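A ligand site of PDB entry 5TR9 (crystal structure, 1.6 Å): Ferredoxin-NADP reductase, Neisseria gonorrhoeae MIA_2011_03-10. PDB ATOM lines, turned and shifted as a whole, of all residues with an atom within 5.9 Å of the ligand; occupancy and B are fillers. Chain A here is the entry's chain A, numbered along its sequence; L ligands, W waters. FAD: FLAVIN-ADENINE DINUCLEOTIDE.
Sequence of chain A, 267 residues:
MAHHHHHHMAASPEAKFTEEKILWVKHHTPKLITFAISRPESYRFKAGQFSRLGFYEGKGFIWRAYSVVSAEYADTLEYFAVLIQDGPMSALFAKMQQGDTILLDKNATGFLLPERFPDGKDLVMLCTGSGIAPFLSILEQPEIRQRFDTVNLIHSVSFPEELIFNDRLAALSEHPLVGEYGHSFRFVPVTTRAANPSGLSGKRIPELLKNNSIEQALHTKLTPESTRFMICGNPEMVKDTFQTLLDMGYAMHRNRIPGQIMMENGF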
ATOM      1  N   PHE A  50      -8.800  25.256  18.181  1.00  0.00           N
ATOM      2  CA  PHE A  50      -8.744  25.012  16.752  1.00  0.00           C
ATOM      3  C   PHE A  50      -8.097  23.668  16.422  1.00  0.00           C
ATOM      4  O   PHE A  50      -7.274  23.125  17.176  1.00  0.00           O
ATOM      5  CB  PHE A  50      -8.020  26.160  16.011  1.00  0.00           C
ATOM      6  CG  PHE A  50      -6.586  26.398  16.422  1.00  0.00           C
ATOM      7  CD1 PHE A  50      -5.538  25.752  15.778  1.00  0.00           C
ATOM      8  CD2 PHE A  50      -6.284  27.333  17.413  1.00  0.00           C
ATOM      9  CE1 PHE A  50      -4.199  26.009  16.142  1.00  0.00           C
ATOM     10  CE2 PHE A  50      -4.960  27.590  17.791  1.00  0.00           C
ATOM     11  CZ  PHE A  50      -3.921  26.923  17.151  1.00  0.00           C
ATOM     12  N   ILE A  62      -0.561  19.380   2.682  1.00  0.00           N
ATOM     13  CA  ILE A  62      -0.843  20.779   3.004  1.00  0.00           C
ATOM     14  C   ILE A  62      -1.689  20.782   4.269  1.00  0.00           C
ATOM     15  O   ILE A  62      -2.603  19.973   4.419  1.00  0.00           O
ATOM     16  CB  ILE A  62      -1.540  21.528   1.844  1.00  0.00           C
ATOM     17  CG1 ILE A  62      -1.751  22.998   2.221  1.00  0.00           C
ATOM     18  CG2 ILE A  62      -2.848  20.851   1.434  1.00  0.00           C
ATOM     19  CD1 ILE A  62      -2.186  23.868   1.046  1.00  0.00           C
ATOM     20  N   ARG A  64      -3.582  23.404   7.391  1.00  0.00           N
ATOM     21  CA  ARG A  64      -4.033  24.716   7.851  1.00  0.00           C
ATOM     22  C   ARG A  64      -4.872  24.578   9.117  1.00  0.00           C
ATOM     23  O   ARG A  64      -5.524  23.549   9.340  1.00  0.00           O
ATOM     24  CB  ARG A  64      -4.864  25.452   6.781  1.00  0.00           C
ATOM     25  CG  ARG A  64      -4.096  25.874   5.524  1.00  0.00           C
ATOM     26  CD  ARG A  64      -3.081  26.967   5.820  1.00  0.00           C
ATOM     27  NE  ARG A  64      -2.520  27.574   4.611  1.00  0.00           N
ATOM     28  CZ  ARG A  64      -1.484  27.083   3.931  1.00  0.00           C
ATOM     29  NH1 ARG A  64      -0.902  25.944   4.307  1.00  0.00           N
ATOM     30  NH2 ARG A  64      -1.035  27.732   2.854  1.00  0.00           N
ATOM     31  N   ALA A  65      -4.900  25.647   9.922  1.00  0.00           N
ATOM     32  CA  ALA A  65      -5.667  25.648  11.169  1.00  0.00           C
ATOM     33  C   ALA A  65      -7.065  26.243  10.961  1.00  0.00           C
ATOM     34  O   ALA A  65      -7.243  27.201  10.202  1.00  0.00           O
ATOM     35  CB  ALA A  65      -4.930  26.456  12.239  1.00  0.00           C
ATOM     36  N   TYR A  66      -8.049  25.664  11.663  1.00  0.00           N
ATOM     37  CA  TYR A  66      -9.449  26.132  11.627  1.00  0.00           C
ATOM     38  C   TYR A  66     -10.060  25.993  12.999  1.00  0.00           C
ATOM     39  O   TYR A  66      -9.950  24.932  13.616  1.00  0.00           O
ATOM     40  CB  TYR A  66     -10.288  25.344  10.609  1.00  0.00           C
ATOM     41  CG  TYR A  66      -9.703  25.533   9.241  1.00  0.00           C
ATOM     42  CD1 TYR A  66     -10.036  26.650   8.466  1.00  0.00           C
ATOM     43  CD2 TYR A  66      -8.769  24.636   8.743  1.00  0.00           C
ATOM     44  CE1 TYR A  66      -9.444  26.865   7.242  1.00  0.00           C
ATOM     45  CE2 TYR A  66      -8.164  24.839   7.534  1.00  0.00           C
ATOM     46  CZ  TYR A  66      -8.513  25.944   6.785  1.00  0.00           C
ATOM     47  OH  TYR A  66      -7.895  26.137   5.575  1.00  0.00           O
ATOM     48  N   SER A  67     -10.723  27.051  13.479  1.00  0.00           N
ATOM     49  CA  SER A  67     -11.428  26.926  14.761  1.00  0.00           C
ATOM     50  C   SER A  67     -12.656  26.028  14.627  1.00  0.00           C
ATOM     51  O   SER A  67     -13.425  26.145  13.672  1.00  0.00           O
ATOM     52  CB  SER A  67     -11.898  28.297  15.247  1.00  0.00           C
ATOM     53  OG  SER A  67     -10.804  29.192  15.366  1.00  0.00           O
ATOM     54  N   VAL A  69     -16.264  25.092  14.909  1.00  0.00           N
ATOM     55  CA  VAL A  69     -17.493  25.861  15.113  1.00  0.00           C
ATOM     56  C   VAL A  69     -18.593  25.012  15.746  1.00  0.00           C
ATOM     57  O   VAL A  69     -19.509  25.574  16.369  1.00  0.00           O
ATOM     58  CB  VAL A  69     -18.010  26.524  13.820  1.00  0.00           C
ATOM     59  CG1 VAL A  69     -16.875  27.230  13.083  1.00  0.00           C
ATOM     60  CG2 VAL A  69     -18.674  25.526  12.914  1.00  0.00           C
ATOM     61  N   PHE A  80     -15.838  26.775   9.582  1.00  0.00           N
ATOM     62  CA  PHE A  80     -16.260  27.919   8.782  1.00  0.00           C
ATOM     63  C   PHE A  80     -15.015  28.466   8.087  1.00  0.00           C
ATOM     64  O   PHE A  80     -14.082  28.902   8.756  1.00  0.00           O
ATOM     65  CB  PHE A  80     -16.897  28.994   9.685  1.00  0.00           C
ATOM     66  CG  PHE A  80     -17.110  30.346   9.026  1.00  0.00           C
ATOM     67  CD1 PHE A  80     -17.468  30.443   7.689  1.00  0.00           C
ATOM     68  CD2 PHE A  80     -17.004  31.515   9.778  1.00  0.00           C
ATOM     69  CE1 PHE A  80     -17.670  31.697   7.099  1.00  0.00           C
ATOM     70  CE2 PHE A  80     -17.235  32.759   9.199  1.00  0.00           C
ATOM     71  CZ  PHE A  80     -17.564  32.854   7.864  1.00  0.00           C
ATOM     72  N   ALA A  81     -15.004  28.426   6.753  1.00  0.00           N
ATOM     73  CA  ALA A  81     -13.852  28.874   5.978  1.00  0.00           C
ATOM     74  C   ALA A  81     -14.223  29.954   4.976  1.00  0.00           C
ATOM     75  O   ALA A  81     -15.258  29.886   4.300  1.00  0.00           O
ATOM     76  CB  ALA A  81     -13.194  27.691   5.230  1.00  0.00           C
ATOM     77  N   VAL A  82     -13.359  30.961   4.885  1.00  0.00           N
ATOM     78  CA  VAL A  82     -13.439  31.974   3.831  1.00  0.00           C
ATOM     79  C   VAL A  82     -12.515  31.562   2.696  1.00  0.00           C
ATOM     80  O   VAL A  82     -11.329  31.287   2.922  1.00  0.00           O
ATOM     81  CB  VAL A  82     -13.088  33.375   4.357  1.00  0.00           C
ATOM     82  CG1 VAL A  82     -11.886  33.317   5.231  1.00  0.00           C
ATOM     83  CG2 VAL A  82     -12.817  34.342   3.200  1.00  0.00           C
ATOM     84  N   ILE A  84     -10.081  32.166  -0.126  1.00  0.00           N
ATOM     85  CA  ILE A  84      -9.159  33.251  -0.420  1.00  0.00           C
ATOM     86  C   ILE A  84      -8.678  33.120  -1.861  1.00  0.00           C
ATOM     87  O   ILE A  84      -8.255  32.026  -2.281  1.00  0.00           O
ATOM     88  CB  ILE A  84      -7.968  33.243   0.551  1.00  0.00           C
ATOM     89  CG1 ILE A  84      -8.449  33.372   2.006  1.00  0.00           C
ATOM     90  CG2 ILE A  84      -6.949  34.322   0.170  1.00  0.00           C
ATOM     91  CD1 ILE A  84      -9.131  34.691   2.297  1.00  0.00           C
ATOM     92  N   ASP A  86      -6.464  32.843  -4.838  1.00  0.00           N
ATOM     93  CA  ASP A  86      -5.132  32.292  -5.050  1.00  0.00           C
ATOM     94  C   ASP A  86      -4.601  31.507  -3.853  1.00  0.00           C
ATOM     95  O   ASP A  86      -3.429  31.096  -3.877  1.00  0.00           O
ATOM     96  CB  ASP A  86      -4.112  33.381  -5.430  1.00  0.00           C
ATOM     97  CG  ASP A  86      -4.556  34.230  -6.600  1.00  0.00           C
ATOM     98  OD1 ASP A  86      -5.131  33.677  -7.565  1.00  0.00           O
ATOM     99  OD2 ASP A  86      -4.328  35.453  -6.554  1.00  0.00           O
ATOM    100  N   GLY A  87      -5.409  31.291  -2.829  1.00  0.00           N
ATOM    101  CA  GLY A  87      -4.967  30.534  -1.671  1.00  0.00           C
ATOM    102  C   GLY A  87      -4.982  29.044  -1.957  1.00  0.00           C
ATOM    103  O   GLY A  87      -5.932  28.510  -2.544  1.00  0.00           O
ATOM    104  N   PRO A  88      -3.912  28.336  -1.581  1.00  0.00           N
ATOM    105  CA  PRO A  88      -3.849  26.901  -1.942  1.00  0.00           C
ATOM    106  C   PRO A  88      -4.855  26.039  -1.219  1.00  0.00           C
ATOM    107  O   PRO A  88      -5.464  25.163  -1.860  1.00  0.00           O
ATOM    108  CB  PRO A  88      -2.398  26.522  -1.603  1.00  0.00           C
ATOM    109  CG  PRO A  88      -1.975  27.527  -0.562  1.00  0.00           C
ATOM    110  CD  PRO A  88      -2.654  28.805  -0.980  1.00  0.00           C
ATOM    111  N   MET A  89      -5.070  26.221   0.087  1.00  0.00           N
ATOM    112  CA  MET A  89      -6.086  25.405   0.757  1.00  0.00           C
ATOM    113  C   MET A  89      -7.477  25.769   0.243  1.00  0.00           C
ATOM    114  O   MET A  89      -8.334  24.888   0.076  1.00  0.00           O
ATOM    115  CB  MET A  89      -6.009  25.574   2.273  1.00  0.00           C
ATOM    116  CG  MET A  89      -6.794  24.489   3.024  1.00  0.00           C
ATOM    117  SD  MET A  89      -5.903  22.919   2.943  1.00  0.00           S
ATOM    118  CE  MET A  89      -6.441  22.130   4.457  1.00  0.00           C
ATOM    119  N   SER A  90      -7.703  27.062  -0.025  1.00  0.00           N
ATOM    120  CA  SER A  90      -8.992  27.500  -0.526  1.00  0.00           C
ATOM    121  C   SER A  90      -9.340  26.821  -1.844  1.00  0.00           C
ATOM    122  O   SER A  90     -10.501  26.462  -2.072  1.00  0.00           O
ATOM    123  CB  SER A  90      -8.999  29.025  -0.686  1.00  0.00           C
ATOM    124  OG  SER A  90      -8.837  29.637   0.585  1.00  0.00           O
ATOM    125  N   ALA A  91      -8.349  26.613  -2.727  1.00  0.00           N
ATOM    126  CA  ALA A  91      -8.615  25.934  -3.983  1.00  0.00           C
ATOM    127  C   ALA A  91      -9.048  24.501  -3.742  1.00  0.00           C
ATOM    128  O   ALA A  91      -9.891  23.965  -4.465  1.00  0.00           O
ATOM    129  CB  ALA A  91      -7.365  25.965  -4.863  1.00  0.00           C
ATOM    130  N   PHE A  93     -10.557  23.421  -0.894  1.00  0.00           N
ATOM    131  CA  PHE A  93     -11.891  23.494  -0.315  1.00  0.00           C
ATOM    132  C   PHE A  93     -12.946  23.716  -1.392  1.00  0.00           C
ATOM    133  O   PHE A  93     -14.063  23.182  -1.292  1.00  0.00           O
ATOM    134  CB  PHE A  93     -11.965  24.632   0.715  1.00  0.00           C
ATOM    135  CG  PHE A  93     -11.334  24.332   2.049  1.00  0.00           C
ATOM    136  CD1 PHE A  93     -10.928  23.053   2.400  1.00  0.00           C
ATOM    137  CD2 PHE A  93     -11.195  25.351   2.981  1.00  0.00           C
ATOM    138  CE1 PHE A  93     -10.389  22.804   3.663  1.00  0.00           C
ATOM    139  CE2 PHE A  93     -10.655  25.113   4.230  1.00  0.00           C
ATOM    140  CZ  PHE A  93     -10.249  23.844   4.582  1.00  0.00           C
ATOM    141  N   SER A 130     -13.975  35.355   9.765  1.00  0.00           N
ATOM    142  CA  SER A 130     -14.058  33.983  10.255  1.00  0.00           C
ATOM    143  C   SER A 130     -13.674  33.852  11.726  1.00  0.00           C
ATOM    144  O   SER A 130     -13.832  32.766  12.295  1.00  0.00           O
ATOM    145  CB  SER A 130     -13.182  33.053   9.402  1.00  0.00           C
ATOM    146  OG  SER A 130     -11.843  33.523   9.339  1.00  0.00           O
ATOM    147  N   GLY A 131     -13.189  34.925  12.357  1.00  0.00           N
ATOM    148  CA  GLY A 131     -12.888  34.932  13.785  1.00  0.00           C
ATOM    149  C   GLY A 131     -14.087  34.685  14.683  1.00  0.00           C
ATOM    150  O   GLY A 131     -13.892  34.437  15.889  1.00  0.00           O
ATOM    151  N   ALA A 133     -15.709  32.033  14.456  1.00  0.00           N
ATOM    152  CA  ALA A 133     -15.780  30.577  14.561  1.00  0.00           C
ATOM    153  C   ALA A 133     -15.591  30.027  15.972  1.00  0.00           C
ATOM    154  O   ALA A 133     -16.464  29.266  16.428  1.00  0.00           O
ATOM    155  CB  ALA A 133     -14.763  29.943  13.596  1.00  0.00           C
ATOM    156  N   PRO A 134     -14.526  30.340  16.709  1.00  0.00           N
ATOM    157  CA  PRO A 134     -14.399  29.759  18.064  1.00  0.00           C
ATOM    158  C   PRO A 134     -15.509  30.199  18.990  1.00  0.00           C
ATOM    159  O   PRO A 134     -15.896  29.452  19.905  1.00  0.00           O
ATOM    160  CB  PRO A 134     -13.033  30.274  18.547  1.00  0.00           C
ATOM    161  CG  PRO A 134     -12.803  31.540  17.750  1.00  0.00           C
ATOM    162  CD  PRO A 134     -13.399  31.247  16.397  1.00  0.00           C
ATOM    163  N   GLU A 264      -6.541  35.954  20.066  1.00  0.00           N
ATOM    164  CA  GLU A 264      -5.938  35.014  19.131  1.00  0.00           C
ATOM    165  C   GLU A 264      -6.127  35.564  17.720  1.00  0.00           C
ATOM    166  O   GLU A 264      -7.251  35.921  17.357  1.00  0.00           O
ATOM    167  CB  GLU A 264      -6.589  33.640  19.279  1.00  0.00           C
ATOM    168  CG  GLU A 264      -6.072  32.553  18.346  1.00  0.00           C
ATOM    169  CD  GLU A 264      -6.869  31.272  18.529  1.00  0.00           C
ATOM    170  OE1 GLU A 264      -7.800  31.029  17.736  1.00  0.00           O
ATOM    171  OE2 GLU A 264      -6.594  30.521  19.500  1.00  0.00           O
ATOM    172  N   ASN A 265      -5.050  35.634  16.933  1.00  0.00           N
ATOM    173  CA  ASN A 265      -5.203  36.060  15.541  1.00  0.00           C
ATOM    174  C   ASN A 265      -6.021  35.013  14.792  1.00  0.00           C
ATOM    175  O   ASN A 265      -5.784  33.811  14.940  1.00  0.00           O
ATOM    176  CB  ASN A 265      -3.837  36.218  14.858  1.00  0.00           C
ATOM    177  CG  ASN A 265      -3.105  37.480  15.295  1.00  0.00           C
ATOM    178  OD1 ASN A 265      -3.634  38.340  15.992  1.00  0.00           O
ATOM    179  ND2 ASN A 265      -1.854  37.589  14.857  1.00  0.00           N
ATOM    180  N   GLY A 266      -6.979  35.476  13.986  1.00  0.00           N
ATOM    181  CA  GLY A 266      -7.839  34.573  13.227  1.00  0.00           C
ATOM    182  C   GLY A 266      -7.209  33.973  11.992  1.00  0.00           C
ATOM    183  O   GLY A 266      -7.791  33.085  11.365  1.00  0.00           O
ATOM    184  N   PHE A 267      -6.042  34.472  11.614  1.00  0.00           N
ATOM    185  CA  PHE A 267      -5.250  33.889  10.547  1.00  0.00           C
ATOM    186  C   PHE A 267      -3.859  34.518  10.580  1.00  0.00           C
ATOM    187  O   PHE A 267      -3.596  35.378  11.434  1.00  0.00           O
ATOM    188  CB  PHE A 267      -5.919  34.094   9.166  1.00  0.00           C
ATOM    189  CG  PHE A 267      -6.188  35.539   8.810  1.00  0.00           C
ATOM    190  CD1 PHE A 267      -5.221  36.312   8.190  1.00  0.00           C
ATOM    191  CD2 PHE A 267      -7.429  36.103   9.050  1.00  0.00           C
ATOM    192  CE1 PHE A 267      -5.468  37.625   7.838  1.00  0.00           C
ATOM    193  CE2 PHE A 267      -7.691  37.417   8.697  1.00  0.00           C
ATOM    194  CZ  PHE A 267      -6.711  38.178   8.091  1.00  0.00           C
ATOM    195  OXT PHE A 267      -2.986  34.177   9.770  1.00  0.00           O
HETATM  196  PA  FAD L   1      -3.091  31.030   2.864  1.00  0.00           P
HETATM  197  O1A FAD L   1      -1.866  30.765   2.047  1.00  0.00           O
HETATM  198  O2A FAD L   1      -3.160  30.347   4.218  1.00  0.00           O
HETATM  199  O5B FAD L   1      -3.301  32.551   3.139  1.00  0.00           O
HETATM  200  C5B FAD L   1      -3.184  33.526   2.079  1.00  0.00           C
HETATM  201  C4B FAD L   1      -3.584  34.864   2.660  1.00  0.00           C
HETATM  202  O4B FAD L   1      -5.013  34.877   2.856  1.00  0.00           O
HETATM  203  C3B FAD L   1      -3.011  35.155   4.047  1.00  0.00           C
HETATM  204  O3B FAD L   1      -1.709  35.718   3.976  1.00  0.00           O
HETATM  205  C2B FAD L   1      -4.015  36.160   4.607  1.00  0.00           C
HETATM  206  O2B FAD L   1      -3.752  37.482   4.138  1.00  0.00           O
HETATM  207  C1B FAD L   1      -5.328  35.686   3.975  1.00  0.00           C
HETATM  208  N9A FAD L   1      -6.190  34.914   4.850  1.00  0.00           N
HETATM  209  C8A FAD L   1      -6.009  33.626   5.279  1.00  0.00           C
HETATM  210  N7A FAD L   1      -6.983  33.163   6.028  1.00  0.00           N
HETATM  211  C5A FAD L   1      -7.883  34.224   6.073  1.00  0.00           C
HETATM  212  C6A FAD L   1      -9.125  34.376   6.715  1.00  0.00           C
HETATM  213  N6A FAD L   1      -9.704  33.424   7.449  1.00  0.00           N
HETATM  214  N1A FAD L   1      -9.760  35.565   6.569  1.00  0.00           N
HETATM  215  C2A FAD L   1      -9.181  36.517   5.835  1.00  0.00           C
HETATM  216  N3A FAD L   1      -8.010  36.489   5.193  1.00  0.00           N
HETATM  217  C4A FAD L   1      -7.412  35.301   5.345  1.00  0.00           C
HETATM  218  N1  FAD L   1      -9.401  30.436   8.342  1.00  0.00           N
HETATM  219  C2  FAD L   1     -10.748  30.277   8.214  1.00  0.00           C
HETATM  220  O2  FAD L   1     -11.322  30.479   7.137  1.00  0.00           O
HETATM  221  N3  FAD L   1     -11.491  29.907   9.335  1.00  0.00           N
HETATM  222  C4  FAD L   1     -10.987  29.690  10.605  1.00  0.00           C
HETATM  223  O4  FAD L   1     -11.730  29.350  11.529  1.00  0.00           O
HETATM  224  C4X FAD L   1      -9.552  29.858  10.711  1.00  0.00           C
HETATM  225  N5  FAD L   1      -8.991  29.676  11.896  1.00  0.00           N
HETATM  226  C5X FAD L   1      -7.626  29.839  11.982  1.00  0.00           C
HETATM  227  C6  FAD L   1      -7.005  29.649  13.220  1.00  0.00           C
HETATM  228  C7  FAD L   1      -5.637  29.805  13.370  1.00  0.00           C
HETATM  229  C7M FAD L   1      -4.996  29.574  14.719  1.00  0.00           C
HETATM  230  C8  FAD L   1      -4.848  30.132  12.255  1.00  0.00           C
HETATM  231  C8M FAD L   1      -3.351  30.295  12.385  1.00  0.00           C
HETATM  232  C9  FAD L   1      -5.454  30.331  11.019  1.00  0.00           C
HETATM  233  C9A FAD L   1      -6.836  30.175  10.868  1.00  0.00           C
HETATM  234  N10 FAD L   1      -7.491  30.405   9.639  1.00  0.00           N
HETATM  235  C10 FAD L   1      -8.841  30.225   9.523  1.00  0.00           C
HETATM  236  C1' FAD L   1      -6.736  30.625   8.405  1.00  0.00           C
HETATM  237  C2' FAD L   1      -6.548  29.280   7.676  1.00  0.00           C
HETATM  238  O2' FAD L   1      -5.637  28.428   8.363  1.00  0.00           O
HETATM  239  C3' FAD L   1      -6.065  29.481   6.238  1.00  0.00           C
HETATM  240  O3' FAD L   1      -4.949  30.378   6.230  1.00  0.00           O
HETATM  241  C4' FAD L   1      -7.165  29.878   5.253  1.00  0.00           C
HETATM  242  O4' FAD L   1      -8.084  28.794   5.128  1.00  0.00           O
HETATM  243  C5' FAD L   1      -6.642  30.251   3.884  1.00  0.00           C
HETATM  244  O5' FAD L   1      -5.810  29.176   3.399  1.00  0.00           O
HETATM  245  P   FAD L   1      -5.155  29.260   1.953  1.00  0.00           P
HETATM  246  O1P FAD L   1      -6.245  29.352   0.891  1.00  0.00           O
HETATM  247  O2P FAD L   1      -4.169  28.150   1.852  1.00  0.00           O
HETATM  248  O3P FAD L   1      -4.386  30.668   2.015  1.00  0.00           O
HETATM  249  O   HOH W   1      -7.419  38.948   4.064  1.00  0.00           O
HETATM  250  O   HOH W   2      -4.968  40.156   4.902  1.00  0.00           O
HETATM  251  O   HOH W   3     -10.523  33.040  11.610  1.00  0.00           O
HETATM  252  O   HOH W   4     -10.530  31.446  13.912  1.00  0.00           O
HETATM  253  O   HOH W   5      -0.514  35.579   6.485  1.00  0.00           O
HETATM  254  O   HOH W   6      -3.091  29.795   8.560  1.00  0.00           O
HETATM  255  O   HOH W   7     -10.375  29.739   4.833  1.00  0.00           O
HETATM  256  O   HOH W   8     -11.893  36.535   7.994  1.00  0.00           O
HETATM  257  O   HOH W   9      -8.129  32.015  15.433  1.00  0.00           O
HETATM  258  O   HOH W  10      -0.104  36.204   1.390  1.00  0.00           O
HETATM  259  O   HOH W  11     -13.625  27.175  11.274  1.00  0.00           O
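An oxygen (O2P) of the ligand sits close to the backbone nitrogen (N) of Pro 88. The backbone carbonyl oxygen of Gly 266 sits close to a nitrogen (N10) of the ligand, at 3.2 Å. Phe 50 touches the ligand. Ala 81 touches the ligand. Ile 84 touches the ligand. CA of Gly 87 touches O1P of the ligand, 3.1 Å away. Ala 133 touches the ligand. CE2 of Phe 267 touches C2A of the ligand (3.3 Å). Hydrophobic or aromatic side chains within 4 Å of the ligand: Phe 50, Ala 65, Tyr 66, Ala 81, Val 82, Ile 84, Pro 88, Met 89, Ala 133 and Phe 267. 17 residues have an atom within 4 Å of the ligand: Phe 50, Arg 64, Ala 65, Tyr 66, Ser 67, Phe 80, Ala 81, Val 82, Ile 84, Gly 87, Pro 88, Met 89, Ser 90, Ser 130, Ala 133, Gly 266 and Phe 267.
The backbone NH (N) of Ile 84 sits at hydrogen-bond distance from the side-chain hydroxyl (OG) of Ser 90 (2.9 Å).
The backbone NH of Ser 90 lies within hydrogen-bond range of an oxygen (O1P) of the ligand (2.9 Å). The side-chain hydroxyl (OG) of Ser 90 sits at hydrogen-bond distance from an oxygen (O1P) of the ligand, 2.6 Å away. OH of Tyr 66 lies within hydrogen-bond range of O4' of the ligand (2.7 Å). The backbone NH (N) of Ala 65 sits at hydrogen-bond distance from an oxygen (O2') of the ligand. An oxygen (O2') of the ligand lies within hydrogen-bond range of the backbone carbonyl oxygen (O) of Ala 65, 2.7 Å away. O2P of the ligand sits at hydrogen-bond distance from N of Met 89, at 2.8 Å. A nitrogen (N3) of the ligand sits at hydrogen-bond distance from the backbone carbonyl oxygen (O) of Phe 80 (2.8 Å). The side-chain hydroxyl of Ser 130 lies within hydrogen-bond range of a nitrogen (N6A) of the ligand, at 2.9 Å. The guanidinium group of Arg 64 lies within salt-bridge range of an oxygen (O2A) of the ligand. The backbone NH of Val 82 sits at hydrogen-bond distance from an oxygen (O2) of the ligand, 3.1 Å away. An oxygen (O4) of the ligand lies within hydrogen-bond range of the backbone NH (N) of Ser 67 (3.2 Å).
Water W7 bridges O4' of the ligand (2.5 Å) and O of Val 82 (2.6 Å). Water W8 lies within hydrogen-bond range of a nitrogen (N1A) of the ligand (2.7 Å) and the backbone NH of Ser 130 (3.0 Å). Water W11 lies within hydrogen-bond range of the backbone carbonyl oxygen of Ser 67 (2.6 Å), the backbone NH of Phe 80 (2.8 Å) and an oxygen (O4) of the ligand (2.9 Å). Water W4 bridges the side-chain hydroxyl of Ser 67 and a nitrogen (N5) of the ligand. Water W9 lies within hydrogen-bond range of OE1 of Glu 264 (2.5 Å) and O of Asn 265 (3.0 Å). Water W3 lies within hydrogen-bond range of OG of Ser 130, O of Gly 266 and N of Gly 131.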
